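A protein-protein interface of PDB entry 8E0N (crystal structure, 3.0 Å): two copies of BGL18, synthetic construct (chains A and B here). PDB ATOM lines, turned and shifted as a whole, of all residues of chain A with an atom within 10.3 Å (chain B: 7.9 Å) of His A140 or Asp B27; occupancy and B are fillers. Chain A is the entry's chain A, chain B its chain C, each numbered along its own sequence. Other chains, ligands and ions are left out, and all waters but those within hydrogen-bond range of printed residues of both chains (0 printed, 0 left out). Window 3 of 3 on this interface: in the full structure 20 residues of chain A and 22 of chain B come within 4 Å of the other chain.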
ATOM      1  N   ALA A  79     -27.290  -9.505 -40.347  1.00  0.00           N
ATOM      2  CA  ALA A  79     -26.444  -8.612 -39.559  1.00  0.00           C
ATOM      3  C   ALA A  79     -25.096  -9.252 -39.251  1.00  0.00           C
ATOM      4  O   ALA A  79     -24.054  -8.590 -39.325  1.00  0.00           O
ATOM      5  CB  ALA A  79     -27.156  -8.216 -38.267  1.00  0.00           C
ATOM      6  N   ARG A  83     -21.353  -7.796 -40.596  1.00  0.00           N
ATOM      7  CA  ARG A  83     -20.249  -7.438 -39.708  1.00  0.00           C
ATOM      8  C   ARG A  83     -18.953  -8.126 -40.133  1.00  0.00           C
ATOM      9  O   ARG A  83     -17.887  -7.501 -40.162  1.00  0.00           O
ATOM     10  CB  ARG A  83     -20.607  -7.798 -38.264  1.00  0.00           C
ATOM     11  N   LEU A  91     -25.927  -3.977 -43.441  1.00  0.00           N
ATOM     12  CA  LEU A  91     -26.344  -3.578 -42.101  1.00  0.00           C
ATOM     13  C   LEU A  91     -27.617  -2.745 -42.145  1.00  0.00           C
ATOM     14  O   LEU A  91     -28.434  -2.807 -41.221  1.00  0.00           O
ATOM     15  CB  LEU A  91     -25.221  -2.801 -41.404  1.00  0.00           C
ATOM     16  CG  LEU A  91     -24.123  -3.598 -40.699  1.00  0.00           C
ATOM     17  CD1 LEU A  91     -22.925  -2.714 -40.394  1.00  0.00           C
ATOM     18  CD2 LEU A  91     -24.659  -4.231 -39.432  1.00  0.00           C
ATOM     19  N   ALA A  95     -31.104  -3.628 -40.381  1.00  0.00           N
ATOM     20  CA  ALA A  95     -31.705  -2.670 -39.461  1.00  0.00           C
ATOM     21  C   ALA A  95     -33.188  -2.481 -39.758  1.00  0.00           C
ATOM     22  O   ALA A  95     -33.998  -2.377 -38.831  1.00  0.00           O
ATOM     23  CB  ALA A  95     -30.963  -1.335 -39.532  1.00  0.00           C
ATOM     24  N   ALA A 132     -34.747  -6.007 -30.409  1.00  0.00           N
ATOM     25  CA  ALA A 132     -33.869  -5.024 -29.783  1.00  0.00           C
ATOM     26  C   ALA A 132     -32.452  -5.557 -29.619  1.00  0.00           C
ATOM     27  O   ALA A 132     -31.487  -4.791 -29.712  1.00  0.00           O
ATOM     28  CB  ALA A 132     -34.436  -4.594 -28.429  1.00  0.00           C
ATOM     29  N   ARG A 133     -32.305  -6.862 -29.381  1.00  0.00           N
ATOM     30  CA  ARG A 133     -30.975  -7.449 -29.263  1.00  0.00           C
ATOM     31  C   ARG A 133     -30.238  -7.400 -30.595  1.00  0.00           C
ATOM     32  O   ARG A 133     -29.018  -7.205 -30.629  1.00  0.00           O
ATOM     33  CB  ARG A 133     -31.089  -8.887 -28.754  1.00  0.00           C
ATOM     34  CG  ARG A 133     -29.766  -9.600 -28.529  1.00  0.00           C
ATOM     35  CD  ARG A 133     -29.994 -11.097 -28.402  1.00  0.00           C
ATOM     36  NE  ARG A 133     -30.791 -11.421 -27.224  1.00  0.00           N
ATOM     37  CZ  ARG A 133     -30.345 -12.079 -26.164  1.00  0.00           C
ATOM     38  NH1 ARG A 133     -29.098 -12.518 -26.095  1.00  0.00           N
ATOM     39  NH2 ARG A 133     -31.170 -12.304 -25.144  1.00  0.00           N
ATOM     40  N   VAL A 134     -30.963  -7.564 -31.702  1.00  0.00           N
ATOM     41  CA  VAL A 134     -30.338  -7.480 -33.019  1.00  0.00           C
ATOM     42  C   VAL A 134     -29.983  -6.034 -33.350  1.00  0.00           C
ATOM     43  O   VAL A 134     -28.887  -5.744 -33.843  1.00  0.00           O
ATOM     44  CB  VAL A 134     -31.257  -8.097 -34.089  1.00  0.00           C
ATOM     45  CG1 VAL A 134     -30.714  -7.818 -35.479  1.00  0.00           C
ATOM     46  CG2 VAL A 134     -31.388  -9.596 -33.860  1.00  0.00           C
ATOM     47  N   LEU A 135     -30.906  -5.104 -33.083  1.00  0.00           N
ATOM     48  CA  LEU A 135     -30.629  -3.690 -33.319  1.00  0.00           C
ATOM     49  C   LEU A 135     -29.463  -3.195 -32.475  1.00  0.00           C
ATOM     50  O   LEU A 135     -28.730  -2.292 -32.895  1.00  0.00           O
ATOM     51  CB  LEU A 135     -31.874  -2.854 -33.024  1.00  0.00           C
ATOM     52  CG  LEU A 135     -33.016  -2.910 -34.039  1.00  0.00           C
ATOM     53  CD1 LEU A 135     -34.127  -1.960 -33.627  1.00  0.00           C
ATOM     54  CD2 LEU A 135     -32.507  -2.554 -35.427  1.00  0.00           C
ATOM     55  N   ALA A 136     -29.280  -3.766 -31.283  1.00  0.00           N
ATOM     56  CA  ALA A 136     -28.183  -3.344 -30.421  1.00  0.00           C
ATOM     57  C   ALA A 136     -26.837  -3.720 -31.026  1.00  0.00           C
ATOM     58  O   ALA A 136     -25.903  -2.909 -31.037  1.00  0.00           O
ATOM     59  CB  ALA A 136     -28.343  -3.959 -29.032  1.00  0.00           C
ATOM     60  N   ARG A 137     -26.717  -4.949 -31.534  1.00  0.00           N
ATOM     61  CA  ARG A 137     -25.475  -5.363 -32.178  1.00  0.00           C
ATOM     62  C   ARG A 137     -25.220  -4.561 -33.445  1.00  0.00           C
ATOM     63  O   ARG A 137     -24.077  -4.184 -33.730  1.00  0.00           O
ATOM     64  CB  ARG A 137     -25.512  -6.857 -32.499  1.00  0.00           C
ATOM     65  CG  ARG A 137     -25.260  -7.766 -31.311  1.00  0.00           C
ATOM     66  CD  ARG A 137     -25.302  -9.230 -31.726  1.00  0.00           C
ATOM     67  NE  ARG A 137     -24.867 -10.112 -30.649  1.00  0.00           N
ATOM     68  CZ  ARG A 137     -24.928 -11.436 -30.691  1.00  0.00           C
ATOM     69  NH1 ARG A 137     -25.404 -12.075 -31.746  1.00  0.00           N
ATOM     70  NH2 ARG A 137     -24.495 -12.137 -29.647  1.00  0.00           N
ATOM     71  N   ILE A 138     -26.271  -4.302 -34.226  1.00  0.00           N
ATOM     72  CA  ILE A 138     -26.113  -3.503 -35.437  1.00  0.00           C
ATOM     73  C   ILE A 138     -25.598  -2.116 -35.081  1.00  0.00           C
ATOM     74  O   ILE A 138     -24.620  -1.632 -35.659  1.00  0.00           O
ATOM     75  CB  ILE A 138     -27.436  -3.436 -36.220  1.00  0.00           C
ATOM     76  CG1 ILE A 138     -27.797  -4.815 -36.777  1.00  0.00           C
ATOM     77  CG2 ILE A 138     -27.346  -2.408 -37.342  1.00  0.00           C
ATOM     78  CD1 ILE A 138     -29.179  -4.880 -37.387  1.00  0.00           C
ATOM     79  N   ALA A 139     -26.227  -1.473 -34.095  1.00  0.00           N
ATOM     80  CA  ALA A 139     -25.799  -0.138 -33.689  1.00  0.00           C
ATOM     81  C   ALA A 139     -24.369  -0.132 -33.165  1.00  0.00           C
ATOM     82  O   ALA A 139     -23.686   0.896 -33.239  1.00  0.00           O
ATOM     83  CB  ALA A 139     -26.752   0.419 -32.635  1.00  0.00           C
ATOM     84  N   HIS A 140     -23.898  -1.260 -32.633  1.00  0.00           N
ATOM     85  CA  HIS A 140     -22.526  -1.332 -32.142  1.00  0.00           C
ATOM     86  C   HIS A 140     -21.528  -1.426 -33.289  1.00  0.00           C
ATOM     87  O   HIS A 140     -20.572  -0.645 -33.356  1.00  0.00           O
ATOM     88  CB  HIS A 140     -22.369  -2.522 -31.195  1.00  0.00           C
ATOM     89  CG  HIS A 140     -20.984  -2.679 -30.648  1.00  0.00           C
ATOM     90  ND1 HIS A 140     -20.229  -1.611 -30.215  1.00  0.00           N
ATOM     91  CD2 HIS A 140     -20.221  -3.781 -30.458  1.00  0.00           C
ATOM     92  CE1 HIS A 140     -19.058  -2.047 -29.786  1.00  0.00           C
ATOM     93  NE2 HIS A 140     -19.028  -3.361 -29.921  1.00  0.00           N
ATOM     94  N   HIS A 141     -21.737  -2.374 -34.202  1.00  0.00           N
ATOM     95  CA  HIS A 141     -20.880  -2.557 -35.370  1.00  0.00           C
ATOM     96  C   HIS A 141     -21.149  -1.526 -36.465  1.00  0.00           C
ATOM     97  O   HIS A 141     -20.784  -1.748 -37.627  1.00  0.00           O
ATOM     98  CB  HIS A 141     -21.055  -3.971 -35.929  1.00  0.00           C
ATOM     99  CG  HIS A 141     -20.377  -5.030 -35.115  1.00  0.00           C
ATOM    100  ND1 HIS A 141     -21.074  -5.962 -34.375  1.00  0.00           N
ATOM    101  CD2 HIS A 141     -19.065  -5.314 -34.936  1.00  0.00           C
ATOM    102  CE1 HIS A 141     -20.221  -6.768 -33.769  1.00  0.00           C
ATOM    103  NE2 HIS A 141     -18.996  -6.398 -34.094  1.00  0.00           N
ATOM    104  N   ARG A 142     -21.778  -0.409 -36.106  1.00  0.00           N
ATOM    105  CA  ARG A 142     -22.125   0.635 -37.056  1.00  0.00           C
ATOM    106  C   ARG A 142     -21.968   2.020 -36.441  1.00  0.00           C
ATOM    107  O   ARG A 142     -22.125   3.021 -37.149  1.00  0.00           O
ATOM    108  CB  ARG A 142     -23.561   0.393 -37.573  1.00  0.00           C
ATOM    109  CG  ARG A 142     -24.183   1.363 -38.570  1.00  0.00           C
ATOM    110  CD  ARG A 142     -25.573   0.829 -38.931  1.00  0.00           C
ATOM    111  NE  ARG A 142     -26.348   1.694 -39.812  1.00  0.00           N
ATOM    112  CZ  ARG A 142     -27.142   2.670 -39.393  1.00  0.00           C
ATOM    113  NH1 ARG A 142     -27.856   3.393 -40.241  1.00  0.00           N
ATOM    114  NH2 ARG A 142     -27.234   2.914 -38.090  1.00  0.00           N
ATOM    115  N   GLY A 143     -21.633   2.105 -35.152  1.00  0.00           N
ATOM    116  CA  GLY A 143     -21.232   3.354 -34.536  1.00  0.00           C
ATOM    117  C   GLY A 143     -22.352   4.313 -34.230  1.00  0.00           C
ATOM    118  O   GLY A 143     -22.091   5.490 -33.964  1.00  0.00           O
ATOM    119  N   ASN A 144     -23.595   3.848 -34.248  1.00  0.00           N
ATOM    120  CA  ASN A 144     -24.755   4.712 -34.073  1.00  0.00           C
ATOM    121  C   ASN A 144     -25.187   4.625 -32.614  1.00  0.00           C
ATOM    122  O   ASN A 144     -25.636   3.571 -32.151  1.00  0.00           O
ATOM    123  CB  ASN A 144     -25.875   4.298 -35.025  1.00  0.00           C
ATOM    124  CG  ASN A 144     -27.063   5.241 -34.985  1.00  0.00           C
ATOM    125  OD1 ASN A 144     -27.201   6.058 -34.075  1.00  0.00           O
ATOM    126  ND2 ASN A 144     -27.927   5.136 -35.987  1.00  0.00           N
ATOM    127  N   GLN A 145     -25.035   5.734 -31.888  1.00  0.00           N
ATOM    128  CA  GLN A 145     -25.417   5.777 -30.482  1.00  0.00           C
ATOM    129  C   GLN A 145     -26.925   5.905 -30.303  1.00  0.00           C
ATOM    130  O   GLN A 145     -27.476   5.373 -29.332  1.00  0.00           O
ATOM    131  CB  GLN A 145     -24.698   6.935 -29.787  1.00  0.00           C
ATOM    132  CG  GLN A 145     -25.008   7.080 -28.309  1.00  0.00           C
ATOM    133  CD  GLN A 145     -24.445   5.946 -27.479  1.00  0.00           C
ATOM    134  OE1 GLN A 145     -23.364   5.429 -27.760  1.00  0.00           O
ATOM    135  NE2 GLN A 145     -25.176   5.556 -26.441  1.00  0.00           N
ATOM    136  N   GLU A 146     -27.605   6.590 -31.225  1.00  0.00           N
ATOM    137  CA  GLU A 146     -29.047   6.772 -31.097  1.00  0.00           C
ATOM    138  C   GLU A 146     -29.792   5.455 -31.275  1.00  0.00           C
ATOM    139  O   GLU A 146     -30.698   5.139 -30.493  1.00  0.00           O
ATOM    140  CB  GLU A 146     -29.536   7.809 -32.109  1.00  0.00           C
ATOM    141  N   LEU A 147     -29.433   4.674 -32.297  1.00  0.00           N
ATOM    142  CA  LEU A 147     -30.065   3.370 -32.482  1.00  0.00           C
ATOM    143  C   LEU A 147     -29.731   2.432 -31.330  1.00  0.00           C
ATOM    144  O   LEU A 147     -30.571   1.626 -30.912  1.00  0.00           O
ATOM    145  CB  LEU A 147     -29.638   2.764 -33.819  1.00  0.00           C
ATOM    146  CG  LEU A 147     -30.036   1.308 -34.067  1.00  0.00           C
ATOM    147  CD1 LEU A 147     -31.536   1.192 -34.277  1.00  0.00           C
ATOM    148  CD2 LEU A 147     -29.281   0.741 -35.259  1.00  0.00           C
ATOM    149  N   LEU A 148     -28.505   2.519 -30.810  1.00  0.00           N
ATOM    150  CA  LEU A 148     -28.156   1.794 -29.593  1.00  0.00           C
ATOM    151  C   LEU A 148     -29.076   2.188 -28.447  1.00  0.00           C
ATOM    152  O   LEU A 148     -29.628   1.329 -27.747  1.00  0.00           O
ATOM    153  CB  LEU A 148     -26.701   2.075 -29.222  1.00  0.00           C
ATOM    154  CG  LEU A 148     -26.296   1.645 -27.813  1.00  0.00           C
ATOM    155  CD1 LEU A 148     -26.462   0.144 -27.655  1.00  0.00           C
ATOM    156  CD2 LEU A 148     -24.883   2.097 -27.483  1.00  0.00           C
ATOM    157  N   GLU A 149     -29.248   3.494 -28.240  1.00  0.00           N
ATOM    158  CA  GLU A 149     -30.144   3.979 -27.200  1.00  0.00           C
ATOM    159  C   GLU A 149     -31.583   3.562 -27.473  1.00  0.00           C
ATOM    160  O   GLU A 149     -32.347   3.320 -26.534  1.00  0.00           O
ATOM    161  CB  GLU A 149     -30.021   5.499 -27.097  1.00  0.00           C
ATOM    162  CG  GLU A 149     -30.861   6.149 -26.018  1.00  0.00           C
ATOM    163  CD  GLU A 149     -30.657   7.650 -25.974  1.00  0.00           C
ATOM    164  OE1 GLU A 149     -29.791   8.151 -26.725  1.00  0.00           O
ATOM    165  OE2 GLU A 149     -31.354   8.330 -25.193  1.00  0.00           O
ATOM    166  N   LYS A 150     -31.966   3.461 -28.749  1.00  0.00           N
ATOM    167  CA  LYS A 150     -33.299   2.975 -29.092  1.00  0.00           C
ATOM    168  C   LYS A 150     -33.481   1.526 -28.662  1.00  0.00           C
ATOM    169  O   LYS A 150     -34.475   1.178 -28.011  1.00  0.00           O
ATOM    170  CB  LYS A 150     -33.543   3.115 -30.595  1.00  0.00           C
ATOM    171  CG  LYS A 150     -35.000   2.945 -30.997  1.00  0.00           C
ATOM    172  CD  LYS A 150     -35.148   2.809 -32.505  1.00  0.00           C
ATOM    173  CE  LYS A 150     -36.317   1.903 -32.869  1.00  0.00           C
ATOM    174  NZ  LYS A 150     -36.630   1.941 -34.324  1.00  0.00           N
ATOM    175  N   ALA A 151     -32.531   0.660 -29.026  1.00  0.00           N
ATOM    176  CA  ALA A 151     -32.644  -0.748 -28.665  1.00  0.00           C
ATOM    177  C   ALA A 151     -32.615  -0.943 -27.156  1.00  0.00           C
ATOM    178  O   ALA A 151     -33.106  -1.961 -26.651  1.00  0.00           O
ATOM    179  CB  ALA A 151     -31.526  -1.550 -29.329  1.00  0.00           C
ATOM    180  N   TRP A 152     -32.055   0.019 -26.422  1.00  0.00           N
ATOM    181  CA  TRP A 152     -31.979  -0.105 -24.971  1.00  0.00           C
ATOM    182  C   TRP A 152     -33.305   0.243 -24.304  1.00  0.00           C
ATOM    183  O   TRP A 152     -33.656  -0.354 -23.279  1.00  0.00           O
ATOM    184  CB  TRP A 152     -30.856   0.772 -24.425  1.00  0.00           C
ATOM    185  CG  TRP A 152     -30.302   0.248 -23.145  1.00  0.00           C
ATOM    186  CD1 TRP A 152     -29.406  -0.770 -22.999  1.00  0.00           C
ATOM    187  CD2 TRP A 152     -30.602   0.711 -21.825  1.00  0.00           C
ATOM    188  NE1 TRP A 152     -29.133  -0.975 -21.671  1.00  0.00           N
ATOM    189  CE2 TRP A 152     -29.852  -0.076 -20.928  1.00  0.00           C
ATOM    190  CE3 TRP A 152     -31.429   1.713 -21.314  1.00  0.00           C
ATOM    191  CZ2 TRP A 152     -29.905   0.107 -19.552  1.00  0.00           C
ATOM    192  CZ3 TRP A 152     -31.479   1.895 -19.947  1.00  0.00           C
ATOM    193  CH2 TRP A 152     -30.722   1.097 -19.083  1.00  0.00           C
ATOM    194  N   THR B  20     -30.320  -9.357 -22.005  1.00  0.00           N
ATOM    195  CA  THR B  20     -30.097  -8.454 -23.129  1.00  0.00           C
ATOM    196  C   THR B  20     -29.510  -7.129 -22.659  1.00  0.00           C
ATOM    197  O   THR B  20     -28.617  -6.573 -23.309  1.00  0.00           O
ATOM    198  CB  THR B  20     -31.407  -8.224 -23.885  1.00  0.00           C
ATOM    199  OG1 THR B  20     -31.976  -9.487 -24.253  1.00  0.00           O
ATOM    200  CG2 THR B  20     -31.166  -7.399 -25.142  1.00  0.00           C
ATOM    201  N   LEU B  21     -29.999  -6.610 -21.530  1.00  0.00           N
ATOM    202  CA  LEU B  21     -29.468  -5.364 -20.987  1.00  0.00           C
ATOM    203  C   LEU B  21     -27.995  -5.504 -20.625  1.00  0.00           C
ATOM    204  O   LEU B  21     -27.175  -4.645 -20.971  1.00  0.00           O
ATOM    205  CB  LEU B  21     -30.291  -4.935 -19.770  1.00  0.00           C
ATOM    206  CG  LEU B  21     -31.683  -4.347 -20.006  1.00  0.00           C
ATOM    207  CD1 LEU B  21     -32.170  -3.646 -18.753  1.00  0.00           C
ATOM    208  CD2 LEU B  21     -31.636  -3.369 -21.168  1.00  0.00           C
ATOM    209  N   ALA B  22     -27.637  -6.588 -19.930  1.00  0.00           N
ATOM    210  CA  ALA B  22     -26.240  -6.797 -19.559  1.00  0.00           C
ATOM    211  C   ALA B  22     -25.359  -6.950 -20.792  1.00  0.00           C
ATOM    212  O   ALA B  22     -24.206  -6.503 -20.799  1.00  0.00           O
ATOM    213  CB  ALA B  22     -26.115  -8.019 -18.649  1.00  0.00           C
ATOM    214  N   GLU B  23     -25.886  -7.576 -21.847  1.00  0.00           N
ATOM    215  CA  GLU B  23     -25.136  -7.699 -23.094  1.00  0.00           C
ATOM    216  C   GLU B  23     -24.848  -6.330 -23.699  1.00  0.00           C
ATOM    217  O   GLU B  23     -23.723  -6.050 -24.127  1.00  0.00           O
ATOM    218  CB  GLU B  23     -25.910  -8.570 -24.084  1.00  0.00           C
ATOM    219  CG  GLU B  23     -25.227  -8.742 -25.428  1.00  0.00           C
ATOM    220  CD  GLU B  23     -25.995  -9.663 -26.356  1.00  0.00           C
ATOM    221  OE1 GLU B  23     -26.031  -9.383 -27.573  1.00  0.00           O
ATOM    222  OE2 GLU B  23     -26.562 -10.665 -25.871  1.00  0.00           O
ATOM    223  N   ILE B  24     -25.864  -5.464 -23.744  1.00  0.00           N
ATOM    224  CA  ILE B  24     -25.693  -4.139 -24.330  1.00  0.00           C
ATOM    225  C   ILE B  24     -24.696  -3.319 -23.520  1.00  0.00           C
ATOM    226  O   ILE B  24     -23.825  -2.642 -24.082  1.00  0.00           O
ATOM    227  CB  ILE B  24     -27.055  -3.431 -24.438  1.00  0.00           C
ATOM    228  CG1 ILE B  24     -27.985  -4.198 -25.381  1.00  0.00           C
ATOM    229  CG2 ILE B  24     -26.873  -2.002 -24.900  1.00  0.00           C
ATOM    230  CD1 ILE B  24     -29.389  -3.635 -25.444  1.00  0.00           C
ATOM    231  N   ALA B  25     -24.805  -3.368 -22.192  1.00  0.00           N
ATOM    232  CA  ALA B  25     -23.881  -2.624 -21.341  1.00  0.00           C
ATOM    233  C   ALA B  25     -22.459  -3.154 -21.466  1.00  0.00           C
ATOM    234  O   ALA B  25     -21.496  -2.378 -21.436  1.00  0.00           O
ATOM    235  CB  ALA B  25     -24.344  -2.688 -19.887  1.00  0.00           C
ATOM    236  N   ARG B  26     -22.309  -4.472 -21.608  1.00  0.00           N
ATOM    237  CA  ARG B  26     -20.981  -5.072 -21.658  1.00  0.00           C
ATOM    238  C   ARG B  26     -20.265  -4.725 -22.958  1.00  0.00           C
ATOM    239  O   ARG B  26     -19.115  -4.274 -22.945  1.00  0.00           O
ATOM    240  CB  ARG B  26     -21.097  -6.586 -21.493  1.00  0.00           C
ATOM    241  CG  ARG B  26     -19.779  -7.331 -21.482  1.00  0.00           C
ATOM    242  CD  ARG B  26     -20.039  -8.817 -21.349  1.00  0.00           C
ATOM    243  NE  ARG B  26     -20.738  -9.122 -20.107  1.00  0.00           N
ATOM    244  CZ  ARG B  26     -21.972  -9.601 -20.040  1.00  0.00           C
ATOM    245  NH1 ARG B  26     -22.551  -9.859 -18.878  1.00  0.00           N
ATOM    246  NH2 ARG B  26     -22.645  -9.822 -21.166  1.00  0.00           N
ATOM    247  N   ASP B  27     -20.937  -4.926 -24.093  1.00  0.00           N
ATOM    248  CA  ASP B  27     -20.322  -4.692 -25.395  1.00  0.00           C
ATOM    249  C   ASP B  27     -20.003  -3.226 -25.646  1.00  0.00           C
ATOM    250  O   ASP B  27     -19.356  -2.915 -26.653  1.00  0.00           O
ATOM    251  CB  ASP B  27     -21.241  -5.212 -26.502  1.00  0.00           C
ATOM    252  CG  ASP B  27     -21.535  -6.692 -26.367  1.00  0.00           C
ATOM    253  OD1 ASP B  27     -20.713  -7.412 -25.761  1.00  0.00           O
ATOM    254  OD2 ASP B  27     -22.594  -7.135 -26.860  1.00  0.00           O
ATOM    255  N   ASN B  28     -20.429  -2.322 -24.765  1.00  0.00           N
ATOM    256  CA  ASN B  28     -20.254  -0.896 -24.984  1.00  0.00           C
ATOM    257  C   ASN B  28     -19.579  -0.194 -23.812  1.00  0.00           C
ATOM    258  O   ASN B  28     -19.501   1.039 -23.806  1.00  0.00           O
ATOM    259  CB  ASN B  28     -21.607  -0.243 -25.288  1.00  0.00           C
ATOM    260  CG  ASN B  28     -22.172  -0.688 -26.620  1.00  0.00           C
ATOM    261  OD1 ASN B  28     -21.428  -1.055 -27.530  1.00  0.00           O
ATOM    262  ND2 ASN B  28     -23.491  -0.683 -26.737  1.00  0.00           N
ATOM    263  N   GLY B  29     -19.093  -0.943 -22.824  1.00  0.00           N
ATOM    264  CA  GLY B  29     -18.327  -0.372 -21.733  1.00  0.00           C
ATOM    265  C   GLY B  29     -19.057   0.699 -20.948  1.00  0.00           C
ATOM    266  O   GLY B  29     -18.491   1.756 -20.649  1.00  0.00           O
ATOM    267  N   ASN B  30     -20.315   0.441 -20.607  1.00  0.00           N
ATOM    268  CA  ASN B  30     -21.145   1.385 -19.866  1.00  0.00           C
ATOM    269  C   ASN B  30     -21.357   0.817 -18.465  1.00  0.00           C
ATOM    270  O   ASN B  30     -22.215  -0.044 -18.256  1.00  0.00           O
ATOM    271  CB  ASN B  30     -22.465   1.628 -20.595  1.00  0.00           C
ATOM    272  CG  ASN B  30     -23.198   2.856 -20.086  1.00  0.00           C
ATOM    273  OD1 ASN B  30     -23.380   3.034 -18.881  1.00  0.00           O
ATOM    274  ND2 ASN B  30     -23.625   3.712 -21.008  1.00  0.00           N
ATOM    275  N   LEU B  34     -24.472  -1.390 -16.729  1.00  0.00           N
ATOM    276  CA  LEU B  34     -24.352  -2.669 -16.038  1.00  0.00           C
ATOM    277  C   LEU B  34     -25.170  -2.672 -14.755  1.00  0.00           C
ATOM    278  O   LEU B  34     -25.835  -3.664 -14.433  1.00  0.00           O
ATOM    279  CB  LEU B  34     -22.885  -2.972 -15.726  1.00  0.00           C
ATOM    280  CG  LEU B  34     -21.951  -3.471 -16.826  1.00  0.00           C
ATOM    281  CD1 LEU B  34     -20.534  -3.591 -16.285  1.00  0.00           C
ATOM    282  CD2 LEU B  34     -22.433  -4.805 -17.368  1.00  0.00           C
ATOM    283  N   ASP B  84     -17.252  -9.251 -15.110  1.00  0.00           N
ATOM    284  CA  ASP B  84     -16.762  -8.204 -15.999  1.00  0.00           C
ATOM    285  C   ASP B  84     -16.572  -6.906 -15.229  1.00  0.00           C
ATOM    286  O   ASP B  84     -16.341  -5.846 -15.820  1.00  0.00           O
ATOM    287  CB  ASP B  84     -17.739  -7.967 -17.147  1.00  0.00           C
ATOM    288  CG  ASP B  84     -17.798  -9.132 -18.119  1.00  0.00           C
ATOM    289  OD1 ASP B  84     -16.737  -9.654 -18.524  1.00  0.00           O
ATOM    290  OD2 ASP B  84     -18.930  -9.508 -18.489  1.00  0.00           O
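Printed residues of chain B within 4 Å of Arg A133: Thr B20 (3.1 Å) and Glu B23 (3.1 Å). Of the printed residues of chain B, Ala A136 touches Ile B24 (3.7 Å). Printed residues of chain B within 4 Å of Arg A137: Glu B23 (3.4 Å). No residue of chain B comes within 4 Å of Ala A139. Printed residues of chain B within 4 Å of Leu A148: Ile B24 (3.5 Å) and Asn B28 (3.2 Å). Glu A149 touches none of the printed residues of chain B. Of the printed residues of chain A, Leu B21 touches Trp A152. Of chain A, only Arg A133 (3.1 Å) and Arg A137 (3.4 Å) come within 4 Å of Glu B23. Of chain A, only His A140 comes within 4 Å of Asp B27. Asn B28 touches two residues of chain A. Leu B34 touches none of the printed residues of chain A. The nearest printed residue of chain B that does not touch His A140 is Arg B26 (7.0 Å). The nearest printed residue of chain B that does not touch Trp A152 is Ala B25 (5.0 Å).
CB of Ala A136 touches CG1 of Ile B24, 3.7 Å away. Ile B24 touches Leu A148. CD2 of Leu A148 touches ND2 of Asn B28, at 3.2 Å. Trp A152 touches Leu B21. CD1 of Trp A152 touches CG2 of Ile B24, at 3.4 Å.
The backbone carbonyl oxygen of Ile B24 lies within hydrogen-bond range of the side-chain amide nitrogen of Asn B28, 3.3 Å away.
Of the 25 printed residues of chain A, 6 touch a printed residue of chain B. Along chain A the printed residues that touch a printed residue of chain B span positions 133 to 152. Printed residues of chain B that touch a printed residue of chain A: Thr B20, Leu B21, Glu B23, Ile B24, Asp B27 and Asn B28. Hydrophobic or aromatic side chains of chain B within 4 Å of the printed part of chain A: Leu B21 and Ile B24. Among the printed residues, 10 pairs touch across the chains.
No position is printed for both chains. Of the 10 pairs that touch across the chains among the printed residues, none has its exchanged pair printed and touching as well.
The side-chain hydroxyl (OG1) of Thr B20 lies within hydrogen-bond range of the guanidinium group (NH2) of Arg A133 (3.1 Å). OE2 of Glu B23 lies within salt-bridge range of NH1 of Arg A133, at 3.1 Å. The guanidinium group of Arg A137 is in salt-bridge range of the side-chain carboxylate of Glu B23, 3.4 Å away. NE2 of His A140 sits close to O of Asp B27 (3.3 Å). OD1 of Asn B28 lies within hydrogen-bond range of ND1 of His A140.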
